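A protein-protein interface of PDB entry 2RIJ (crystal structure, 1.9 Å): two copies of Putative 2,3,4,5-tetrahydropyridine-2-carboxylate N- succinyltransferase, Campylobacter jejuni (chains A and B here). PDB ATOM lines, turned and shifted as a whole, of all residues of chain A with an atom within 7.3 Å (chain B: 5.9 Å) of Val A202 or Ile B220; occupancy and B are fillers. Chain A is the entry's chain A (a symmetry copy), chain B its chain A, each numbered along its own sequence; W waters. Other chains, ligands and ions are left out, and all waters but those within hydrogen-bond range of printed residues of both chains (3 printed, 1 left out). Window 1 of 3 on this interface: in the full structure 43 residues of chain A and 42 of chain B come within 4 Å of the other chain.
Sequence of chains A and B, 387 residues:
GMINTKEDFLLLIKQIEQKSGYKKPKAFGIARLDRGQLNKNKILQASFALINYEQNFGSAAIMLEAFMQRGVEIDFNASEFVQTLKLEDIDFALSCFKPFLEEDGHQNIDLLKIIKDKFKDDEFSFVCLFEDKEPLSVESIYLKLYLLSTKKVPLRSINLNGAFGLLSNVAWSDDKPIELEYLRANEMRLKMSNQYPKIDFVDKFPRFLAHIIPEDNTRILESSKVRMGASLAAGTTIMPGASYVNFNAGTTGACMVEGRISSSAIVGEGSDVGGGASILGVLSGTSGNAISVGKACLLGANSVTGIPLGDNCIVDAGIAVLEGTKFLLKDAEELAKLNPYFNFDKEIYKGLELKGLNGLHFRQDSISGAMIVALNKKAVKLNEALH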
ATOM      1  N   ASN A 169      17.354  11.018 -29.680  1.00  0.00           N
ATOM      2  CA  ASN A 169      16.455  10.830 -28.541  1.00  0.00           C
ATOM      3  C   ASN A 169      15.522  12.031 -28.490  1.00  0.00           C
ATOM      4  O   ASN A 169      15.962  13.171 -28.348  1.00  0.00           O
ATOM      5  CB  ASN A 169      17.241  10.694 -27.224  1.00  0.00           C
ATOM      6  CG  ASN A 169      16.365  10.329 -26.048  1.00  0.00           C
ATOM      7  OD1 ASN A 169      15.382   9.586 -26.201  1.00  0.00           O
ATOM      8  ND2 ASN A 169      16.687  10.866 -24.863  1.00  0.00           N
ATOM      9  N   VAL A 170      14.232  11.762 -28.604  1.00  0.00           N
ATOM     10  CA  VAL A 170      13.216  12.823 -28.678  1.00  0.00           C
ATOM     11  C   VAL A 170      12.046  12.447 -27.781  1.00  0.00           C
ATOM     12  O   VAL A 170      11.886  11.284 -27.400  1.00  0.00           O
ATOM     13  CB  VAL A 170      12.736  13.091 -30.134  1.00  0.00           C
ATOM     14  CG1 VAL A 170      13.925  13.574 -31.039  1.00  0.00           C
ATOM     15  CG2 VAL A 170      12.064  11.849 -30.745  1.00  0.00           C
ATOM     16  N   ALA A 171      11.250  13.454 -27.472  1.00  0.00           N
ATOM     17  CA  ALA A 171       9.933  13.286 -26.840  1.00  0.00           C
ATOM     18  C   ALA A 171       8.933  12.942 -27.925  1.00  0.00           C
ATOM     19  O   ALA A 171       9.105  13.346 -29.079  1.00  0.00           O
ATOM     20  CB  ALA A 171       9.529  14.560 -26.116  1.00  0.00           C
ATOM     21  N   TRP A 172       7.892  12.197 -27.545  1.00  0.00           N
ATOM     22  CA  TRP A 172       6.880  11.732 -28.475  1.00  0.00           C
ATOM     23  C   TRP A 172       5.547  12.044 -27.861  1.00  0.00           C
ATOM     24  O   TRP A 172       5.294  11.738 -26.683  1.00  0.00           O
ATOM     25  CB  TRP A 172       7.001  10.243 -28.755  1.00  0.00           C
ATOM     26  CG  TRP A 172       8.277   9.823 -29.335  1.00  0.00           C
ATOM     27  CD1 TRP A 172       9.405   9.503 -28.653  1.00  0.00           C
ATOM     28  CD2 TRP A 172       8.567   9.613 -30.721  1.00  0.00           C
ATOM     29  NE1 TRP A 172      10.387   9.124 -29.520  1.00  0.00           N
ATOM     30  CE2 TRP A 172       9.912   9.177 -30.801  1.00  0.00           C
ATOM     31  CE3 TRP A 172       7.842   9.781 -31.902  1.00  0.00           C
ATOM     32  CZ2 TRP A 172      10.541   8.893 -32.013  1.00  0.00           C
ATOM     33  CZ3 TRP A 172       8.464   9.463 -33.121  1.00  0.00           C
ATOM     34  CH2 TRP A 172       9.807   9.046 -33.163  1.00  0.00           C
ATOM     35  N   ILE A 178       9.184  15.460 -30.813  1.00  0.00           N
ATOM     36  CA  ILE A 178       9.515  16.821 -30.415  1.00  0.00           C
ATOM     37  C   ILE A 178      10.909  16.810 -29.808  1.00  0.00           C
ATOM     38  O   ILE A 178      11.191  16.031 -28.906  1.00  0.00           O
ATOM     39  CB  ILE A 178       8.526  17.340 -29.360  1.00  0.00           C
ATOM     40  CG1 ILE A 178       7.088  17.163 -29.856  1.00  0.00           C
ATOM     41  CG2 ILE A 178       8.887  18.819 -28.937  1.00  0.00           C
ATOM     42  CD1 ILE A 178       6.023  17.525 -28.834  1.00  0.00           C
ATOM     43  N   LEU A 180      13.804  17.570 -27.426  1.00  0.00           N
ATOM     44  CA  LEU A 180      13.820  17.874 -26.004  1.00  0.00           C
ATOM     45  C   LEU A 180      14.219  19.351 -25.785  1.00  0.00           C
ATOM     46  O   LEU A 180      13.675  20.020 -24.916  1.00  0.00           O
ATOM     47  CB  LEU A 180      14.755  16.904 -25.232  1.00  0.00           C
ATOM     48  CG  LEU A 180      14.249  15.430 -25.220  1.00  0.00           C
ATOM     49  CD1 LEU A 180      15.330  14.474 -24.735  1.00  0.00           C
ATOM     50  CD2 LEU A 180      12.983  15.296 -24.395  1.00  0.00           C
ATOM     51  N   LEU A 183      11.306  21.654 -25.951  1.00  0.00           N
ATOM     52  CA  LEU A 183      10.513  21.638 -24.750  1.00  0.00           C
ATOM     53  C   LEU A 183      11.174  22.470 -23.666  1.00  0.00           C
ATOM     54  O   LEU A 183      10.506  23.197 -22.929  1.00  0.00           O
ATOM     55  CB  LEU A 183      10.278  20.189 -24.274  1.00  0.00           C
ATOM     56  CG  LEU A 183       9.372  19.286 -25.087  1.00  0.00           C
ATOM     57  CD1 LEU A 183       9.414  17.862 -24.489  1.00  0.00           C
ATOM     58  CD2 LEU A 183       7.911  19.775 -25.169  1.00  0.00           C
ATOM     59  N   ILE A 199       3.384  14.183 -23.279  1.00  0.00           N
ATOM     60  CA  ILE A 199       4.538  13.383 -23.692  1.00  0.00           C
ATOM     61  C   ILE A 199       4.301  11.932 -23.285  1.00  0.00           C
ATOM     62  O   ILE A 199       4.253  11.589 -22.109  1.00  0.00           O
ATOM     63  CB  ILE A 199       5.861  13.965 -23.127  1.00  0.00           C
ATOM     64  CG1 ILE A 199       6.027  15.449 -23.550  1.00  0.00           C
ATOM     65  CG2 ILE A 199       7.068  13.074 -23.502  1.00  0.00           C
ATOM     66  CD1 ILE A 199       5.949  15.716 -25.061  1.00  0.00           C
ATOM     67  N   ASP A 200       4.150  11.072 -24.281  1.00  0.00           N
ATOM     68  CA  ASP A 200       3.912   9.664 -24.017  1.00  0.00           C
ATOM     69  C   ASP A 200       5.176   8.865 -23.688  1.00  0.00           C
ATOM     70  O   ASP A 200       5.110   7.877 -22.944  1.00  0.00           O
ATOM     71  CB  ASP A 200       3.182   9.049 -25.191  1.00  0.00           C
ATOM     72  CG  ASP A 200       1.822   9.680 -25.390  1.00  0.00           C
ATOM     73  OD1 ASP A 200       1.097   9.910 -24.383  1.00  0.00           O
ATOM     74  OD2 ASP A 200       1.530  10.001 -26.544  1.00  0.00           O
ATOM     75  N   PHE A 201       6.302   9.240 -24.295  1.00  0.00           N
ATOM     76  CA  PHE A 201       7.579   8.573 -24.101  1.00  0.00           C
ATOM     77  C   PHE A 201       8.735   9.418 -24.654  1.00  0.00           C
ATOM     78  O   PHE A 201       8.529  10.376 -25.401  1.00  0.00           O
ATOM     79  CB  PHE A 201       7.597   7.128 -24.633  1.00  0.00           C
ATOM     80  CG  PHE A 201       7.482   6.962 -26.152  1.00  0.00           C
ATOM     81  CD1 PHE A 201       6.271   7.082 -26.790  1.00  0.00           C
ATOM     82  CD2 PHE A 201       8.577   6.642 -26.905  1.00  0.00           C
ATOM     83  CE1 PHE A 201       6.152   6.922 -28.162  1.00  0.00           C
ATOM     84  CE2 PHE A 201       8.466   6.438 -28.259  1.00  0.00           C
ATOM     85  CZ  PHE A 201       7.252   6.588 -28.900  1.00  0.00           C
ATOM     86  N   VAL A 202       9.926   9.087 -24.216  1.00  0.00           N
ATOM     87  CA  VAL A 202      11.189   9.736 -24.669  1.00  0.00           C
ATOM     88  C   VAL A 202      12.138   8.612 -25.072  1.00  0.00           C
ATOM     89  O   VAL A 202      12.505   7.751 -24.240  1.00  0.00           O
ATOM     90  CB  VAL A 202      11.816  10.667 -23.601  1.00  0.00           C
ATOM     91  CG1 VAL A 202      13.259  11.239 -24.083  1.00  0.00           C
ATOM     92  CG2 VAL A 202      10.810  11.754 -23.155  1.00  0.00           C
ATOM     93  N   ASP A 203      12.476   8.572 -26.366  1.00  0.00           N
ATOM     94  CA  ASP A 203      13.302   7.515 -26.899  1.00  0.00           C
ATOM     95  C   ASP A 203      13.732   7.857 -28.319  1.00  0.00           C
ATOM     96  O   ASP A 203      13.267   8.838 -28.957  1.00  0.00           O
ATOM     97  CB  ASP A 203      12.531   6.175 -26.925  1.00  0.00           C
ATOM     98  CG  ASP A 203      13.425   4.955 -27.217  1.00  0.00           C
ATOM     99  OD1 ASP A 203      14.656   5.016 -27.012  1.00  0.00           O
ATOM    100  OD2 ASP A 203      12.884   3.930 -27.704  1.00  0.00           O
ATOM    101  N   LYS A 204      14.622   7.036 -28.812  1.00  0.00           N
ATOM    102  CA  LYS A 204      15.128   7.116 -30.189  1.00  0.00           C
ATOM    103  C   LYS A 204      14.279   6.377 -31.231  1.00  0.00           C
ATOM    104  O   LYS A 204      14.430   6.635 -32.424  1.00  0.00           O
ATOM    105  CB  LYS A 204      16.582   6.574 -30.252  1.00  0.00           C
ATOM    106  CG  LYS A 204      17.612   7.492 -29.586  1.00  0.00           C
ATOM    107  CD  LYS A 204      18.980   6.864 -29.535  1.00  0.00           C
ATOM    108  CE  LYS A 204      20.061   7.906 -29.178  1.00  0.00           C
ATOM    109  NZ  LYS A 204      21.415   7.397 -29.331  1.00  0.00           N
ATOM    110  N   PHE A 205      13.452   5.437 -30.791  1.00  0.00           N
ATOM    111  CA  PHE A 205      12.623   4.621 -31.678  1.00  0.00           C
ATOM    112  C   PHE A 205      11.138   4.923 -31.435  1.00  0.00           C
ATOM    113  O   PHE A 205      10.731   5.090 -30.279  1.00  0.00           O
ATOM    114  CB  PHE A 205      12.802   3.128 -31.396  1.00  0.00           C
ATOM    115  CG  PHE A 205      14.093   2.540 -31.883  1.00  0.00           C
ATOM    116  CD1 PHE A 205      15.283   2.846 -31.236  1.00  0.00           C
ATOM    117  CD2 PHE A 205      14.116   1.649 -32.934  1.00  0.00           C
ATOM    118  CE1 PHE A 205      16.510   2.314 -31.681  1.00  0.00           C
ATOM    119  CE2 PHE A 205      15.344   1.106 -33.382  1.00  0.00           C
ATOM    120  CZ  PHE A 205      16.535   1.484 -32.764  1.00  0.00           C
ATOM    121  N   ARG A 207       6.956   3.461 -31.991  1.00  0.00           N
ATOM    122  CA  ARG A 207       6.253   2.240 -31.790  1.00  0.00           C
ATOM    123  C   ARG A 207       5.792   1.695 -33.149  1.00  0.00           C
ATOM    124  O   ARG A 207       5.512   2.444 -34.090  1.00  0.00           O
ATOM    125  CB  ARG A 207       5.091   2.460 -30.836  1.00  0.00           C
ATOM    126  CG  ARG A 207       5.621   2.793 -29.410  1.00  0.00           C
ATOM    127  CD  ARG A 207       4.728   3.539 -28.592  1.00  0.00           C
ATOM    128  NE  ARG A 207       5.279   3.753 -27.259  1.00  0.00           N
ATOM    129  CZ  ARG A 207       4.566   4.247 -26.283  1.00  0.00           C
ATOM    130  NH1 ARG A 207       3.324   4.580 -26.506  1.00  0.00           N
ATOM    131  NH2 ARG A 207       5.080   4.386 -25.096  1.00  0.00           N
ATOM    132  N   PHE B 208       5.529  11.429 -14.268  1.00  0.00           N
ATOM    133  CA  PHE B 208       6.785  12.207 -14.436  1.00  0.00           C
ATOM    134  C   PHE B 208       6.828  13.028 -15.710  1.00  0.00           C
ATOM    135  O   PHE B 208       7.138  14.209 -15.649  1.00  0.00           O
ATOM    136  CB  PHE B 208       7.943  11.185 -14.354  1.00  0.00           C
ATOM    137  CG  PHE B 208       9.328  11.709 -14.501  1.00  0.00           C
ATOM    138  CD1 PHE B 208       9.886  11.859 -15.767  1.00  0.00           C
ATOM    139  CD2 PHE B 208      10.161  11.877 -13.369  1.00  0.00           C
ATOM    140  CE1 PHE B 208      11.220  12.229 -15.927  1.00  0.00           C
ATOM    141  CE2 PHE B 208      11.482  12.242 -13.522  1.00  0.00           C
ATOM    142  CZ  PHE B 208      12.009  12.453 -14.821  1.00  0.00           C
ATOM    143  N   LEU B 209       6.463  12.433 -16.854  1.00  0.00           N
ATOM    144  CA  LEU B 209       6.592  13.129 -18.118  1.00  0.00           C
ATOM    145  C   LEU B 209       5.527  14.222 -18.318  1.00  0.00           C
ATOM    146  O   LEU B 209       5.629  15.012 -19.230  1.00  0.00           O
ATOM    147  CB  LEU B 209       6.665  12.122 -19.297  1.00  0.00           C
ATOM    148  CG  LEU B 209       7.989  11.361 -19.422  1.00  0.00           C
ATOM    149  CD1 LEU B 209       7.796  10.255 -20.511  1.00  0.00           C
ATOM    150  CD2 LEU B 209       9.189  12.290 -19.750  1.00  0.00           C
ATOM    151  N   PRO B 214      13.336  14.973 -19.525  1.00  0.00           N
ATOM    152  CA  PRO B 214      14.586  14.231 -19.297  1.00  0.00           C
ATOM    153  C   PRO B 214      15.795  14.901 -19.959  1.00  0.00           C
ATOM    154  O   PRO B 214      15.628  15.699 -20.879  1.00  0.00           O
ATOM    155  CB  PRO B 214      14.323  12.907 -20.019  1.00  0.00           C
ATOM    156  CG  PRO B 214      12.877  12.724 -19.980  1.00  0.00           C
ATOM    157  CD  PRO B 214      12.343  14.112 -20.217  1.00  0.00           C
ATOM    158  N   GLU B 215      16.972  14.541 -19.491  1.00  0.00           N
ATOM    159  CA  GLU B 215      18.249  14.917 -20.128  1.00  0.00           C
ATOM    160  C   GLU B 215      18.279  14.261 -21.488  1.00  0.00           C
ATOM    161  O   GLU B 215      17.515  13.319 -21.781  1.00  0.00           O
ATOM    162  CB  GLU B 215      19.418  14.395 -19.303  1.00  0.00           C
ATOM    163  CG  GLU B 215      19.535  15.012 -17.915  1.00  0.00           C
ATOM    164  CD  GLU B 215      18.785  14.235 -16.823  1.00  0.00           C
ATOM    165  OE1 GLU B 215      18.008  13.286 -17.129  1.00  0.00           O
ATOM    166  OE2 GLU B 215      18.981  14.594 -15.644  1.00  0.00           O
ATOM    167  N   THR B 218      18.633  10.458 -21.387  1.00  0.00           N
ATOM    168  CA  THR B 218      17.702   9.733 -20.533  1.00  0.00           C
ATOM    169  C   THR B 218      16.497   9.373 -21.343  1.00  0.00           C
ATOM    170  O   THR B 218      15.910  10.190 -22.072  1.00  0.00           O
ATOM    171  CB  THR B 218      17.325  10.558 -19.325  1.00  0.00           C
ATOM    172  OG1 THR B 218      18.509  10.819 -18.597  1.00  0.00           O
ATOM    173  CG2 THR B 218      16.295   9.865 -18.437  1.00  0.00           C
ATOM    174  N   ARG B 219      16.129   8.109 -21.251  1.00  0.00           N
ATOM    175  CA  ARG B 219      14.964   7.595 -22.009  1.00  0.00           C
ATOM    176  C   ARG B 219      13.941   6.942 -21.110  1.00  0.00           C
ATOM    177  O   ARG B 219      14.302   6.190 -20.192  1.00  0.00           O
ATOM    178  CB  ARG B 219      15.469   6.621 -23.045  1.00  0.00           C
ATOM    179  CG  ARG B 219      16.515   7.249 -23.956  1.00  0.00           C
ATOM    180  CD  ARG B 219      16.949   6.322 -25.078  1.00  0.00           C
ATOM    181  NE  ARG B 219      17.770   5.228 -24.576  1.00  0.00           N
ATOM    182  CZ  ARG B 219      17.783   3.969 -24.989  1.00  0.00           C
ATOM    183  NH1 ARG B 219      16.964   3.497 -25.927  1.00  0.00           N
ATOM    184  NH2 ARG B 219      18.650   3.146 -24.421  1.00  0.00           N
ATOM    185  N   ILE B 220      12.662   7.203 -21.391  1.00  0.00           N
ATOM    186  CA  ILE B 220      11.557   6.598 -20.672  1.00  0.00           C
ATOM    187  C   ILE B 220      10.628   6.128 -21.749  1.00  0.00           C
ATOM    188  O   ILE B 220       9.966   6.951 -22.449  1.00  0.00           O
ATOM    189  CB  ILE B 220      10.835   7.601 -19.786  1.00  0.00           C
ATOM    190  CG1 ILE B 220      11.760   8.136 -18.703  1.00  0.00           C
ATOM    191  CG2 ILE B 220       9.530   7.011 -19.262  1.00  0.00           C
ATOM    192  CD1 ILE B 220      11.213   9.410 -17.984  1.00  0.00           C
ATOM    193  N   LEU B 221      10.577   4.828 -21.961  1.00  0.00           N
ATOM    194  CA  LEU B 221       9.873   4.283 -23.169  1.00  0.00           C
ATOM    195  C   LEU B 221       8.366   4.179 -23.030  1.00  0.00           C
ATOM    196  O   LEU B 221       7.682   3.831 -23.987  1.00  0.00           O
ATOM    197  CB  LEU B 221      10.484   2.936 -23.619  1.00  0.00           C
ATOM    198  CG  LEU B 221      11.683   3.045 -24.570  1.00  0.00           C
ATOM    199  CD1 LEU B 221      12.856   3.694 -23.872  1.00  0.00           C
ATOM    200  CD2 LEU B 221      12.035   1.649 -25.169  1.00  0.00           C
ATOM    201  N   GLU B 222       7.851   4.518 -21.855  1.00  0.00           N
ATOM    202  CA  GLU B 222       6.419   4.582 -21.620  1.00  0.00           C
ATOM    203  C   GLU B 222       6.157   5.372 -20.348  1.00  0.00           C
ATOM    204  O   GLU B 222       6.636   5.017 -19.257  1.00  0.00           O
ATOM    205  CB  GLU B 222       5.782   3.185 -21.529  1.00  0.00           C
ATOM    206  CG  GLU B 222       4.304   3.128 -21.046  1.00  0.00           C
ATOM    207  CD  GLU B 222       3.385   4.259 -21.595  1.00  0.00           C
ATOM    208  OE1 GLU B 222       3.530   4.609 -22.803  1.00  0.00           O
ATOM    209  OE2 GLU B 222       2.520   4.823 -20.827  1.00  0.00           O
ATOM    210  N   SER B 223       5.399   6.450 -20.499  1.00  0.00           N
ATOM    211  CA  SER B 223       5.115   7.365 -19.404  1.00  0.00           C
ATOM    212  C   SER B 223       4.467   6.718 -18.181  1.00  0.00           C
ATOM    213  O   SER B 223       4.797   7.076 -17.094  1.00  0.00           O
ATOM    214  CB  SER B 223       4.226   8.547 -19.857  1.00  0.00           C
ATOM    215  OG  SER B 223       4.059   9.515 -18.817  1.00  0.00           O
ATOM    216  N   LYS B 225       5.088   4.201 -16.680  1.00  0.00           N
ATOM    217  CA  LYS B 225       6.078   3.458 -15.888  1.00  0.00           C
ATOM    218  C   LYS B 225       6.952   4.315 -14.958  1.00  0.00           C
ATOM    219  O   LYS B 225       7.744   3.760 -14.213  1.00  0.00           O
ATOM    220  CB  LYS B 225       6.996   2.657 -16.792  1.00  0.00           C
ATOM    221  CG  LYS B 225       6.331   1.587 -17.671  1.00  0.00           C
ATOM    222  CD  LYS B 225       5.156   0.894 -16.949  1.00  0.00           C
ATOM    223  CE  LYS B 225       4.623  -0.337 -17.723  1.00  0.00           C
ATOM    224  NZ  LYS B 225       5.580  -1.469 -17.518  1.00  0.00           N
ATOM    225  N   VAL B 226       6.812   5.631 -15.035  1.00  0.00           N
ATOM    226  CA  VAL B 226       7.532   6.564 -14.147  1.00  0.00           C
ATOM    227  C   VAL B 226       6.559   7.534 -13.512  1.00  0.00           C
ATOM    228  O   VAL B 226       6.028   8.452 -14.160  1.00  0.00           O
ATOM    229  CB  VAL B 226       8.688   7.280 -14.871  1.00  0.00           C
ATOM    230  CG1 VAL B 226       9.536   8.139 -13.875  1.00  0.00           C
ATOM    231  CG2 VAL B 226       9.586   6.268 -15.602  1.00  0.00           C
ATOM    232  N   LEU B 232      15.505  10.086 -11.753  1.00  0.00           N
ATOM    233  CA  LEU B 232      16.316   9.337 -12.703  1.00  0.00           C
ATOM    234  C   LEU B 232      17.605  10.092 -13.036  1.00  0.00           C
ATOM    235  O   LEU B 232      17.559  11.170 -13.615  1.00  0.00           O
ATOM    236  CB  LEU B 232      15.505   9.095 -13.961  1.00  0.00           C
ATOM    237  CG  LEU B 232      14.089   8.492 -13.805  1.00  0.00           C
ATOM    238  CD1 LEU B 232      13.528   8.255 -15.231  1.00  0.00           C
ATOM    239  CD2 LEU B 232      14.088   7.190 -12.935  1.00  0.00           C
ATOM    240  N   THR B 236      19.902   7.281 -17.543  1.00  0.00           N
ATOM    241  CA  THR B 236      19.037   6.121 -17.266  1.00  0.00           C
ATOM    242  C   THR B 236      18.090   5.793 -18.429  1.00  0.00           C
ATOM    243  O   THR B 236      17.614   6.708 -19.109  1.00  0.00           O
ATOM    244  CB  THR B 236      18.240   6.435 -15.977  1.00  0.00           C
ATOM    245  OG1 THR B 236      19.186   6.566 -14.892  1.00  0.00           O
ATOM    246  CG2 THR B 236      17.166   5.349 -15.613  1.00  0.00           C
ATOM    247  N   THR B 237      17.806   4.502 -18.632  1.00  0.00           N
ATOM    248  CA  THR B 237      16.791   3.991 -19.566  1.00  0.00           C
ATOM    249  C   THR B 237      15.747   3.198 -18.794  1.00  0.00           C
ATOM    250  O   THR B 237      16.070   2.254 -18.048  1.00  0.00           O
ATOM    251  CB  THR B 237      17.414   3.089 -20.652  1.00  0.00           C
ATOM    252  OG1 THR B 237      18.461   3.806 -21.320  1.00  0.00           O
ATOM    253  CG2 THR B 237      16.393   2.602 -21.682  1.00  0.00           C
ATOM    254  N   ILE B 238      14.501   3.587 -18.949  1.00  0.00           N
ATOM    255  CA  ILE B 238      13.356   2.795 -18.460  1.00  0.00           C
ATOM    256  C   ILE B 238      12.667   2.120 -19.646  1.00  0.00           C
ATOM    257  O   ILE B 238      12.015   2.768 -20.500  1.00  0.00           O
ATOM    258  CB  ILE B 238      12.316   3.635 -17.703  1.00  0.00           C
ATOM    259  CG1 ILE B 238      13.013   4.612 -16.697  1.00  0.00           C
ATOM    260  CG2 ILE B 238      11.282   2.737 -17.006  1.00  0.00           C
ATOM    261  CD1 ILE B 238      13.869   3.866 -15.629  1.00  0.00           C
HETATM  262  O   HOH W   1       8.144   3.039 -26.564  1.00  0.00           O
HETATM  263  O   HOH W   2       2.833  11.621 -19.779  1.00  0.00           O
HETATM  264  O   HOH W   3       3.672  15.952 -21.050  1.00  0.00           O
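The side-chain amide nitrogen (ND2) of Asn A169 is in hydrogen-bond range of the backbone carbonyl oxygen (O) of Thr B218 (3.0 Å). OD1 of Asp A203 is in salt-bridge range of NH1 of Arg B219 (3.0 Å). O of Ile B220 is in hydrogen-bond range of N of Val A202 (2.8 Å). The side-chain carboxylate (OE1) of Glu B222 is in salt-bridge range of the guanidinium group (NH2) of Arg A207 (2.8 Å). N of Ser B223 is in hydrogen-bond range of O of Asp A200 (2.8 Å). O of Leu B221 sits at hydrogen-bond distance from NH2 of Arg A207, at 2.9 Å.
Water W2 bridges the side-chain hydroxyl of Ser B223 (2.6 Å) and the backbone carbonyl oxygen of Ile A199 (2.7 Å). Water W1 bridges O of Leu B221 (2.7 Å) and NE of Arg A207 (3.0 Å). Water W3 bridges O of Leu B209 (2.8 Å) and N of Ile A199 (2.9 Å).
Among the printed residues, pairs that only touch across the chains: Phe A201 with Ile B220 (3.2 Å), Val A202 with Arg B219 (3.3 Å), Phe A201 with Leu B221 (3.4 Å), Asn A169 with Arg B219 (3.4 Å), Asp A203 with Leu B221 (3.5 Å), Val A202 with Thr B218 (3.5 Å), Asp A200 with Glu B222 (3.6 Å), Ile A199 with Leu B209 (3.7 Å), Ile A199 with Ser B223 (3.8 Å), Val A202 with Leu B209 (3.8 Å), Phe A201 with Glu B222 (3.8 Å), Leu A180 with Glu B215 (3.9 Å), Val A202 with Pro B214 (3.9 Å) and Phe A201 with Leu B209 (3.97 Å).
O of Trp A172 lies within hydrogen-bond range of N of Asp A200 (2.7 Å). The side-chain carboxylate of Asp A203 lies close to the backbone NH of Phe A205 (3.5 Å). The backbone carbonyl oxygen (O) of Arg B219 is in hydrogen-bond range of the backbone NH (N) of Ile B238, at 2.9 Å. The side-chain amide oxygen (OD1) of Asn A169 lies close to the backbone NH (N) of Asp A203, 3.1 Å away. N of Asp A203 is in hydrogen-bond range of O of Val A170, 3.0 Å away. O of Ile B238 lies within hydrogen-bond range of N of Leu B221 (2.9 Å).
Of the printed residues of chain B, Leu A180 touches Glu B215. Of the printed residues of chain B, Arg A207 touches Leu B221 (2.9 Å) and Glu B222 (2.8 Å). Of the printed residues of chain A, Glu B215 touches Leu A180. Of the printed residues of chain A, Thr B218 touches Asn A169 and Val A202. Ile B220 touches just these residues of chain A: Phe A201 and Val A202. Printed residues of chain A within 4 Å of Ser B223: Ile A199 (3.8 Å) and Asp A200 (2.8 Å).
Printed residues of chain A that touch a printed residue of chain B: Asn A169, Leu A180, Ile A199, Asp A200, Phe A201, Val A202, Asp A203 and Arg A207. Of the 16 printed residues of chain B, 9 touch a printed residue of chain A. Hydrophobic or aromatic side chains of chain B within 4 Å of the printed part of chain A: Leu B209, Pro B214 and Leu B221. Among the printed residues, 20 pairs touch across the chains.
No position is printed for both chains. Of the 20 pairs that touch across the chains among the printed residues, none has its exchanged pair printed and touching as well.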
